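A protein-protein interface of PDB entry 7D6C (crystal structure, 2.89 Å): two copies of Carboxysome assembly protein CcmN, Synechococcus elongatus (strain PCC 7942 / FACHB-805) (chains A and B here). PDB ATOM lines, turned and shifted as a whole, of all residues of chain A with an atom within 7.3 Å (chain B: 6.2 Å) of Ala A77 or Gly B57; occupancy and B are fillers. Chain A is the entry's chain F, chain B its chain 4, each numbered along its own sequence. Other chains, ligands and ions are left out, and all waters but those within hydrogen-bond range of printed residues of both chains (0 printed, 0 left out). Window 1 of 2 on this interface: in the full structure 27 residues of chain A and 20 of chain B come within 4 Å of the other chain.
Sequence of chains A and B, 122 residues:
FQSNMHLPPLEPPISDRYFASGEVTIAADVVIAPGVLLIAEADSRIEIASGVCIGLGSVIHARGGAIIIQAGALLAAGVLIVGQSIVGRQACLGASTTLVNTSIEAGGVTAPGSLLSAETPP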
ATOM      1  N   LEU A  10       0.345  -1.284 -14.021  1.00  0.00           N
ATOM      2  CA  LEU A  10       0.618  -2.327 -13.047  1.00  0.00           C
ATOM      3  C   LEU A  10      -0.644  -2.552 -12.221  1.00  0.00           C
ATOM      4  O   LEU A  10      -1.036  -1.687 -11.434  1.00  0.00           O
ATOM      5  CB  LEU A  10       1.805  -1.909 -12.192  1.00  0.00           C
ATOM      6  CG  LEU A  10       2.080  -2.493 -10.824  1.00  0.00           C
ATOM      7  CD1 LEU A  10       2.335  -3.989 -10.905  1.00  0.00           C
ATOM      8  CD2 LEU A  10       3.281  -1.732 -10.255  1.00  0.00           C
ATOM      9  N   GLU A  11      -1.278  -3.708 -12.392  1.00  0.00           N
ATOM     10  CA  GLU A  11      -2.611  -3.863 -11.818  1.00  0.00           C
ATOM     11  C   GLU A  11      -2.573  -4.366 -10.367  1.00  0.00           C
ATOM     12  O   GLU A  11      -1.636  -5.061  -9.959  1.00  0.00           O
ATOM     13  CB  GLU A  11      -3.431  -4.831 -12.668  1.00  0.00           C
ATOM     14  CG  GLU A  11      -3.534  -4.488 -14.159  1.00  0.00           C
ATOM     15  CD  GLU A  11      -4.638  -3.475 -14.476  1.00  0.00           C
ATOM     16  OE1 GLU A  11      -4.422  -2.592 -15.351  1.00  0.00           O
ATOM     17  OE2 GLU A  11      -5.715  -3.568 -13.841  1.00  0.00           O
ATOM     18  N   PRO A  13      -3.637  -6.725  -7.061  1.00  0.00           N
ATOM     19  CA  PRO A  13      -3.981  -8.141  -6.959  1.00  0.00           C
ATOM     20  C   PRO A  13      -5.453  -8.333  -6.621  1.00  0.00           C
ATOM     21  O   PRO A  13      -6.117  -7.450  -6.076  1.00  0.00           O
ATOM     22  CB  PRO A  13      -3.074  -8.640  -5.827  1.00  0.00           C
ATOM     23  CG  PRO A  13      -2.841  -7.448  -4.988  1.00  0.00           C
ATOM     24  CD  PRO A  13      -2.775  -6.297  -5.940  1.00  0.00           C
ATOM     25  N   ALA A  33       5.184 -11.323  -3.455  1.00  0.00           N
ATOM     26  CA  ALA A  33       3.981 -10.498  -3.443  1.00  0.00           C
ATOM     27  C   ALA A  33       2.789 -11.269  -4.007  1.00  0.00           C
ATOM     28  O   ALA A  33       2.955 -12.202  -4.803  1.00  0.00           O
ATOM     29  CB  ALA A  33       4.192  -9.230  -4.253  1.00  0.00           C
ATOM     30  N   VAL A  36       1.891 -12.940  -7.938  1.00  0.00           N
ATOM     31  CA  VAL A  36       3.026 -13.395  -8.725  1.00  0.00           C
ATOM     32  C   VAL A  36       2.771 -14.812  -9.239  1.00  0.00           C
ATOM     33  O   VAL A  36       2.112 -15.635  -8.587  1.00  0.00           O
ATOM     34  CB  VAL A  36       4.311 -13.290  -7.900  1.00  0.00           C
ATOM     35  CG1 VAL A  36       5.441 -14.046  -8.575  1.00  0.00           C
ATOM     36  CG2 VAL A  36       4.661 -11.825  -7.731  1.00  0.00           C
ATOM     37  N   ILE A  54      10.098 -10.831  -4.480  1.00  0.00           N
ATOM     38  CA  ILE A  54       9.515 -10.722  -5.808  1.00  0.00           C
ATOM     39  C   ILE A  54       8.308  -9.812  -5.730  1.00  0.00           C
ATOM     40  O   ILE A  54       7.340 -10.112  -5.018  1.00  0.00           O
ATOM     41  CB  ILE A  54       9.116 -12.086  -6.371  1.00  0.00           C
ATOM     42  CG1 ILE A  54      10.316 -13.062  -6.261  1.00  0.00           C
ATOM     43  CG2 ILE A  54       8.514 -11.897  -7.790  1.00  0.00           C
ATOM     44  CD1 ILE A  54       9.977 -14.480  -6.552  1.00  0.00           C
ATOM     45  N   GLY A  55       8.348  -8.734  -6.505  1.00  0.00           N
ATOM     46  CA  GLY A  55       7.321  -7.719  -6.439  1.00  0.00           C
ATOM     47  C   GLY A  55       6.039  -8.064  -7.177  1.00  0.00           C
ATOM     48  O   GLY A  55       5.978  -8.922  -8.064  1.00  0.00           O
ATOM     49  N   LEU A  56       4.999  -7.343  -6.768  1.00  0.00           N
ATOM     50  CA  LEU A  56       3.670  -7.390  -7.368  1.00  0.00           C
ATOM     51  C   LEU A  56       3.702  -7.614  -8.878  1.00  0.00           C
ATOM     52  O   LEU A  56       4.502  -7.009  -9.599  1.00  0.00           O
ATOM     53  CB  LEU A  56       2.964  -6.069  -7.065  1.00  0.00           C
ATOM     54  CG  LEU A  56       1.506  -6.058  -7.450  1.00  0.00           C
ATOM     55  CD1 LEU A  56       0.862  -7.299  -6.844  1.00  0.00           C
ATOM     56  CD2 LEU A  56       0.856  -4.773  -6.959  1.00  0.00           C
ATOM     57  N   GLY A  57       2.812  -8.478  -9.358  1.00  0.00           N
ATOM     58  CA  GLY A  57       2.641  -8.630 -10.792  1.00  0.00           C
ATOM     59  C   GLY A  57       3.796  -9.255 -11.548  1.00  0.00           C
ATOM     60  O   GLY A  57       3.830  -9.166 -12.781  1.00  0.00           O
ATOM     61  N   SER A  58       4.752  -9.879 -10.861  1.00  0.00           N
ATOM     62  CA  SER A  58       5.856 -10.492 -11.583  1.00  0.00           C
ATOM     63  C   SER A  58       5.418 -11.844 -12.114  1.00  0.00           C
ATOM     64  O   SER A  58       4.427 -12.420 -11.663  1.00  0.00           O
ATOM     65  CB  SER A  58       7.087 -10.625 -10.692  1.00  0.00           C
ATOM     66  OG  SER A  58       7.668  -9.360 -10.404  1.00  0.00           O
ATOM     67  N   VAL A  59       6.122 -12.324 -13.128  1.00  0.00           N
ATOM     68  CA  VAL A  59       5.781 -13.606 -13.733  1.00  0.00           C
ATOM     69  C   VAL A  59       7.077 -14.318 -14.063  1.00  0.00           C
ATOM     70  O   VAL A  59       7.886 -13.807 -14.848  1.00  0.00           O
ATOM     71  CB  VAL A  59       4.919 -13.466 -14.997  1.00  0.00           C
ATOM     72  CG1 VAL A  59       4.799 -14.825 -15.725  1.00  0.00           C
ATOM     73  CG2 VAL A  59       3.541 -12.898 -14.646  1.00  0.00           C
ATOM     74  N   LEU A  75      13.325  -8.360  -7.174  1.00  0.00           N
ATOM     75  CA  LEU A  75      12.585  -8.094  -8.396  1.00  0.00           C
ATOM     76  C   LEU A  75      11.511  -7.070  -8.071  1.00  0.00           C
ATOM     77  O   LEU A  75      10.642  -7.332  -7.231  1.00  0.00           O
ATOM     78  CB  LEU A  75      11.953  -9.376  -8.937  1.00  0.00           C
ATOM     79  CG  LEU A  75      12.724 -10.333  -9.850  1.00  0.00           C
ATOM     80  CD1 LEU A  75      13.996 -10.809  -9.202  1.00  0.00           C
ATOM     81  CD2 LEU A  75      11.828 -11.515 -10.118  1.00  0.00           C
ATOM     82  N   ALA A  76      11.568  -5.911  -8.728  1.00  0.00           N
ATOM     83  CA  ALA A  76      10.491  -4.939  -8.590  1.00  0.00           C
ATOM     84  C   ALA A  76       9.228  -5.493  -9.228  1.00  0.00           C
ATOM     85  O   ALA A  76       9.223  -6.576  -9.817  1.00  0.00           O
ATOM     86  CB  ALA A  76      10.870  -3.607  -9.226  1.00  0.00           C
ATOM     87  N   ALA A  77       8.143  -4.735  -9.118  1.00  0.00           N
ATOM     88  CA  ALA A  77       6.861  -5.190  -9.640  1.00  0.00           C
ATOM     89  C   ALA A  77       6.937  -5.485 -11.137  1.00  0.00           C
ATOM     90  O   ALA A  77       7.698  -4.857 -11.882  1.00  0.00           O
ATOM     91  CB  ALA A  77       5.785  -4.136  -9.377  1.00  0.00           C
ATOM     92  N   GLY A  78       6.148  -6.468 -11.573  1.00  0.00           N
ATOM     93  CA  GLY A  78       5.999  -6.765 -12.993  1.00  0.00           C
ATOM     94  C   GLY A  78       7.245  -7.207 -13.745  1.00  0.00           C
ATOM     95  O   GLY A  78       7.290  -7.099 -14.972  1.00  0.00           O
ATOM     96  N   VAL A  79       8.266  -7.701 -13.052  1.00  0.00           N
ATOM     97  CA  VAL A  79       9.386  -8.323 -13.744  1.00  0.00           C
ATOM     98  C   VAL A  79       8.917  -9.615 -14.410  1.00  0.00           C
ATOM     99  O   VAL A  79       8.097 -10.366 -13.855  1.00  0.00           O
ATOM    100  CB  VAL A  79      10.529  -8.564 -12.749  1.00  0.00           C
ATOM    101  CG1 VAL A  79      11.697  -9.320 -13.408  1.00  0.00           C
ATOM    102  CG2 VAL A  79      10.981  -7.241 -12.213  1.00  0.00           C
ATOM    103  N   LEU A  80       9.425  -9.874 -15.616  1.00  0.00           N
ATOM    104  CA  LEU A  80       9.017 -11.030 -16.405  1.00  0.00           C
ATOM    105  C   LEU A  80      10.241 -11.837 -16.823  1.00  0.00           C
ATOM    106  O   LEU A  80      11.124 -11.321 -17.519  1.00  0.00           O
ATOM    107  CB  LEU A  80       8.234 -10.584 -17.631  1.00  0.00           C
ATOM    108  CG  LEU A  80       8.035 -11.728 -18.593  1.00  0.00           C
ATOM    109  CD1 LEU A  80       6.954 -12.605 -18.033  1.00  0.00           C
ATOM    110  CD2 LEU A  80       7.667 -11.191 -19.948  1.00  0.00           C
ATOM    111  N   LEU A  93      16.343  -5.790 -10.022  1.00  0.00           N
ATOM    112  CA  LEU A  93      15.681  -5.730 -11.322  1.00  0.00           C
ATOM    113  C   LEU A  93      14.574  -4.684 -11.270  1.00  0.00           C
ATOM    114  O   LEU A  93      13.587  -4.859 -10.545  1.00  0.00           O
ATOM    115  CB  LEU A  93      15.115  -7.091 -11.700  1.00  0.00           C
ATOM    116  CG  LEU A  93      16.050  -8.297 -11.707  1.00  0.00           C
ATOM    117  CD1 LEU A  93      15.355  -9.429 -12.455  1.00  0.00           C
ATOM    118  CD2 LEU A  93      17.346  -7.944 -12.352  1.00  0.00           C
ATOM    119  N   GLY A  94      14.735  -3.611 -12.051  1.00  0.00           N
ATOM    120  CA  GLY A  94      13.748  -2.552 -12.060  1.00  0.00           C
ATOM    121  C   GLY A  94      12.375  -3.049 -12.463  1.00  0.00           C
ATOM    122  O   GLY A  94      12.219  -4.111 -13.057  1.00  0.00           O
ATOM    123  N   ALA A  95      11.362  -2.261 -12.108  1.00  0.00           N
ATOM    124  CA  ALA A  95       9.995  -2.543 -12.526  1.00  0.00           C
ATOM    125  C   ALA A  95       9.912  -2.835 -14.021  1.00  0.00           C
ATOM    126  O   ALA A  95      10.535  -2.162 -14.848  1.00  0.00           O
ATOM    127  CB  ALA A  95       9.086  -1.361 -12.178  1.00  0.00           C
ATOM    128  N   SER A  96       9.144  -3.868 -14.354  1.00  0.00           N
ATOM    129  CA  SER A  96       8.861  -4.250 -15.738  1.00  0.00           C
ATOM    130  C   SER A  96      10.123  -4.546 -16.546  1.00  0.00           C
ATOM    131  O   SER A  96      10.154  -4.363 -17.768  1.00  0.00           O
ATOM    132  CB  SER A  96       8.011  -3.190 -16.417  1.00  0.00           C
ATOM    133  OG  SER A  96       6.873  -2.972 -15.602  1.00  0.00           O
ATOM    134  N   THR A  97      11.163  -5.019 -15.869  1.00  0.00           N
ATOM    135  CA  THR A  97      12.232  -5.726 -16.552  1.00  0.00           C
ATOM    136  C   THR A  97      11.679  -6.960 -17.251  1.00  0.00           C
ATOM    137  O   THR A  97      10.821  -7.667 -16.713  1.00  0.00           O
ATOM    138  CB  THR A  97      13.301  -6.164 -15.549  1.00  0.00           C
ATOM    139  OG1 THR A  97      13.784  -5.032 -14.824  1.00  0.00           O
ATOM    140  CG2 THR A  97      14.453  -6.859 -16.267  1.00  0.00           C
ATOM    141  N   ALA B  33      -0.068   1.558  -0.593  1.00  0.00           N
ATOM    142  CA  ALA B  33      -0.885   0.883  -1.596  1.00  0.00           C
ATOM    143  C   ALA B  33      -0.843  -0.640  -1.428  1.00  0.00           C
ATOM    144  O   ALA B  33      -0.037  -1.184  -0.661  1.00  0.00           O
ATOM    145  CB  ALA B  33      -0.415   1.286  -2.986  1.00  0.00           C
ATOM    146  N   PRO B  34      -1.707  -1.360  -2.139  1.00  0.00           N
ATOM    147  CA  PRO B  34      -1.713  -2.824  -2.017  1.00  0.00           C
ATOM    148  C   PRO B  34      -0.500  -3.476  -2.658  1.00  0.00           C
ATOM    149  O   PRO B  34       0.075  -2.984  -3.632  1.00  0.00           O
ATOM    150  CB  PRO B  34      -3.000  -3.236  -2.739  1.00  0.00           C
ATOM    151  CG  PRO B  34      -3.837  -2.011  -2.756  1.00  0.00           C
ATOM    152  CD  PRO B  34      -2.884  -0.872  -2.877  1.00  0.00           C
ATOM    153  N   GLY B  35      -0.121  -4.618  -2.088  1.00  0.00           N
ATOM    154  CA  GLY B  35       0.979  -5.402  -2.605  1.00  0.00           C
ATOM    155  C   GLY B  35       2.323  -4.772  -2.407  1.00  0.00           C
ATOM    156  O   GLY B  35       3.285  -5.187  -3.053  1.00  0.00           O
ATOM    157  N   VAL B  36       2.422  -3.766  -1.558  1.00  0.00           N
ATOM    158  CA  VAL B  36       3.723  -3.185  -1.257  1.00  0.00           C
ATOM    159  C   VAL B  36       4.470  -4.129  -0.334  1.00  0.00           C
ATOM    160  O   VAL B  36       3.876  -4.783   0.534  1.00  0.00           O
ATOM    161  CB  VAL B  36       3.574  -1.791  -0.627  1.00  0.00           C
ATOM    162  CG1 VAL B  36       4.903  -1.305  -0.057  1.00  0.00           C
ATOM    163  CG2 VAL B  36       2.995  -0.800  -1.654  1.00  0.00           C
ATOM    164  N   LEU B  37       5.775  -4.227  -0.548  1.00  0.00           N
ATOM    165  CA  LEU B  37       6.679  -4.963   0.317  1.00  0.00           C
ATOM    166  C   LEU B  37       7.568  -3.961   1.032  1.00  0.00           C
ATOM    167  O   LEU B  37       8.165  -3.080   0.399  1.00  0.00           O
ATOM    168  CB  LEU B  37       7.520  -5.944  -0.492  1.00  0.00           C
ATOM    169  CG  LEU B  37       6.707  -6.845  -1.421  1.00  0.00           C
ATOM    170  CD1 LEU B  37       7.616  -7.831  -2.109  1.00  0.00           C
ATOM    171  CD2 LEU B  37       5.556  -7.557  -0.718  1.00  0.00           C
ATOM    172  N   GLY B  55       3.106   4.166  -3.630  1.00  0.00           N
ATOM    173  CA  GLY B  55       2.309   3.629  -4.706  1.00  0.00           C
ATOM    174  C   GLY B  55       2.330   2.115  -4.750  1.00  0.00           C
ATOM    175  O   GLY B  55       3.150   1.423  -4.138  1.00  0.00           O
ATOM    176  N   LEU B  56       1.389   1.609  -5.535  1.00  0.00           N
ATOM    177  CA  LEU B  56       1.162   0.183  -5.681  1.00  0.00           C
ATOM    178  C   LEU B  56       2.410  -0.598  -6.098  1.00  0.00           C
ATOM    179  O   LEU B  56       3.261  -0.114  -6.852  1.00  0.00           O
ATOM    180  CB  LEU B  56      -0.029  -0.006  -6.631  1.00  0.00           C
ATOM    181  CG  LEU B  56      -0.455  -1.394  -7.037  1.00  0.00           C
ATOM    182  CD1 LEU B  56      -1.920  -1.537  -7.067  1.00  0.00           C
ATOM    183  CD2 LEU B  56      -0.048  -1.394  -8.471  1.00  0.00           C
ATOM    184  N   GLY B  57       2.541  -1.796  -5.518  1.00  0.00           N
ATOM    185  CA  GLY B  57       3.604  -2.725  -5.847  1.00  0.00           C
ATOM    186  C   GLY B  57       4.996  -2.335  -5.413  1.00  0.00           C
ATOM    187  O   GLY B  57       5.939  -3.089  -5.669  1.00  0.00           O
ATOM    188  N   SER B  58       5.170  -1.188  -4.772  1.00  0.00           N
ATOM    189  CA  SER B  58       6.524  -0.734  -4.479  1.00  0.00           C
ATOM    190  C   SER B  58       7.211  -1.697  -3.524  1.00  0.00           C
ATOM    191  O   SER B  58       6.573  -2.337  -2.684  1.00  0.00           O
ATOM    192  CB  SER B  58       6.512   0.687  -3.900  1.00  0.00           C
ATOM    193  OG  SER B  58       6.234   1.643  -4.915  1.00  0.00           O
ATOM    194  N   VAL B  59       8.524  -1.811  -3.679  1.00  0.00           N
ATOM    195  CA  VAL B  59       9.350  -2.701  -2.868  1.00  0.00           C
ATOM    196  C   VAL B  59      10.473  -1.870  -2.238  1.00  0.00           C
ATOM    197  O   VAL B  59      11.269  -1.237  -2.950  1.00  0.00           O
ATOM    198  CB  VAL B  59       9.926  -3.872  -3.694  1.00  0.00           C
ATOM    199  CG1 VAL B  59      10.896  -4.642  -2.873  1.00  0.00           C
ATOM    200  CG2 VAL B  59       8.837  -4.815  -4.166  1.00  0.00           C
ATOM    201  N   ALA B  77       3.867   4.073  -8.322  1.00  0.00           N
ATOM    202  CA  ALA B  77       3.757   2.624  -8.405  1.00  0.00           C
ATOM    203  C   ALA B  77       5.051   2.018  -8.940  1.00  0.00           C
ATOM    204  O   ALA B  77       5.746   2.612  -9.767  1.00  0.00           O
ATOM    205  CB  ALA B  77       2.586   2.215  -9.295  1.00  0.00           C
ATOM    206  N   GLY B  78       5.378   0.818  -8.446  1.00  0.00           N
ATOM    207  CA  GLY B  78       6.542   0.133  -8.953  1.00  0.00           C
ATOM    208  C   GLY B  78       7.864   0.707  -8.511  1.00  0.00           C
ATOM    209  O   GLY B  78       8.891   0.429  -9.127  1.00  0.00           O
ATOM    210  N   VAL B  79       7.890   1.491  -7.445  1.00  0.00           N
ATOM    211  CA  VAL B  79       9.175   1.963  -6.950  1.00  0.00           C
ATOM    212  C   VAL B  79       9.938   0.806  -6.295  1.00  0.00           C
ATOM    213  O   VAL B  79       9.355  -0.128  -5.725  1.00  0.00           O
ATOM    214  CB  VAL B  79       8.954   3.146  -5.987  1.00  0.00           C
ATOM    215  CG1 VAL B  79      10.194   3.501  -5.254  1.00  0.00           C
ATOM    216  CG2 VAL B  79       8.504   4.357  -6.770  1.00  0.00           C
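The backbone NH (N) of Gly B78 lies within hydrogen-bond range of the backbone carbonyl oxygen (O) of Leu B56 (2.8 Å). The backbone NH (N) of Val B59 lies within hydrogen-bond range of the backbone carbonyl oxygen (O) of Val B79. The backbone carbonyl oxygen of Gly A55 is in hydrogen-bond range of the side-chain hydroxyl of Ser A58. The backbone carbonyl oxygen of Leu A75 sits at hydrogen-bond distance from the backbone NH of Gly A55. O of Leu A56 sits at hydrogen-bond distance from N of Gly A78 (2.6 Å). The backbone NH (N) of Ser A96 sits at hydrogen-bond distance from the backbone carbonyl oxygen (O) of Ala A77 (3.0 Å).
Gly A55 touches Val B59, but with the chains exchanged Val A59 does not touch Gly B55 (16.7 Å). Leu A56 touches its own counterpart, Leu B56. Leu A56 touches Gly B57, but with the chains exchanged Gly A57 does not touch Leu B56 (7.7 Å). Ala A77 touches Gly B57, but with the chains exchanged Gly A57 does not touch Ala B77 (10.7 Å). Positions printed for both chains: 33, 36, 55, 56, 57, 58, 59, 77, 78 and 79.
Ala A77 touches just one residue of chain B: Gly B57. Gly B57 touches two residues of chain A. Of the printed residues of chain A, Leu B56 touches Leu A10 and Leu A56. Printed residues of chain A within 4 Å of Gly B78: Leu A10 and Ala A95. Of the printed residues of chain B, Leu A10 touches Leu B56 (3.1 Å) and Gly B78 (3.8 Å). Gly B35 touches none of the printed residues of chain A. Leu A93 touches none of the printed residues of chain B. The nearest residue of chain B that does not touch Ala A77 is Gly B78 (4.4 Å).
Printed residues of chain B that touch a printed residue of chain A: Pro B34, Leu B37, Leu B56, Gly B57, Val B59 and Gly B78. Hydrophobic or aromatic side chains of chain B that line the printed part of chain A: Leu B37, Leu B56 and Val B59. Of the 22 printed residues of chain A, 6 touch a printed residue of chain B. Printed residues of chain A that touch a printed residue of chain B: Leu A10, Ile A54, Gly A55, Leu A56, Ala A77 and Ala A95. Hydrophobic or aromatic side chains of chain A within 4 Å of the printed part of chain B: Leu A10, Leu A56, Ala A77 and Ala A95.
Leu A10 touches Leu B56 (O to CD2, 3.1 Å). CD2 of Leu A10 touches N of Gly B78, 3.8 Å away. Ile A54 touches Leu B37. Gly A55 touches Val B59 (CA to CG2, 3.99 Å). CD2 of Leu A56 touches O of Pro B34, at 3.9 Å. Leu B56 touches Leu A56 (CG to CD2, 3.6 Å). Gly B57 touches Leu A56 (CA to CD2, 3.6 Å). Gly B57 touches Ala A77 (O to CB, 3.9 Å). Ala A95 touches Gly B78.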
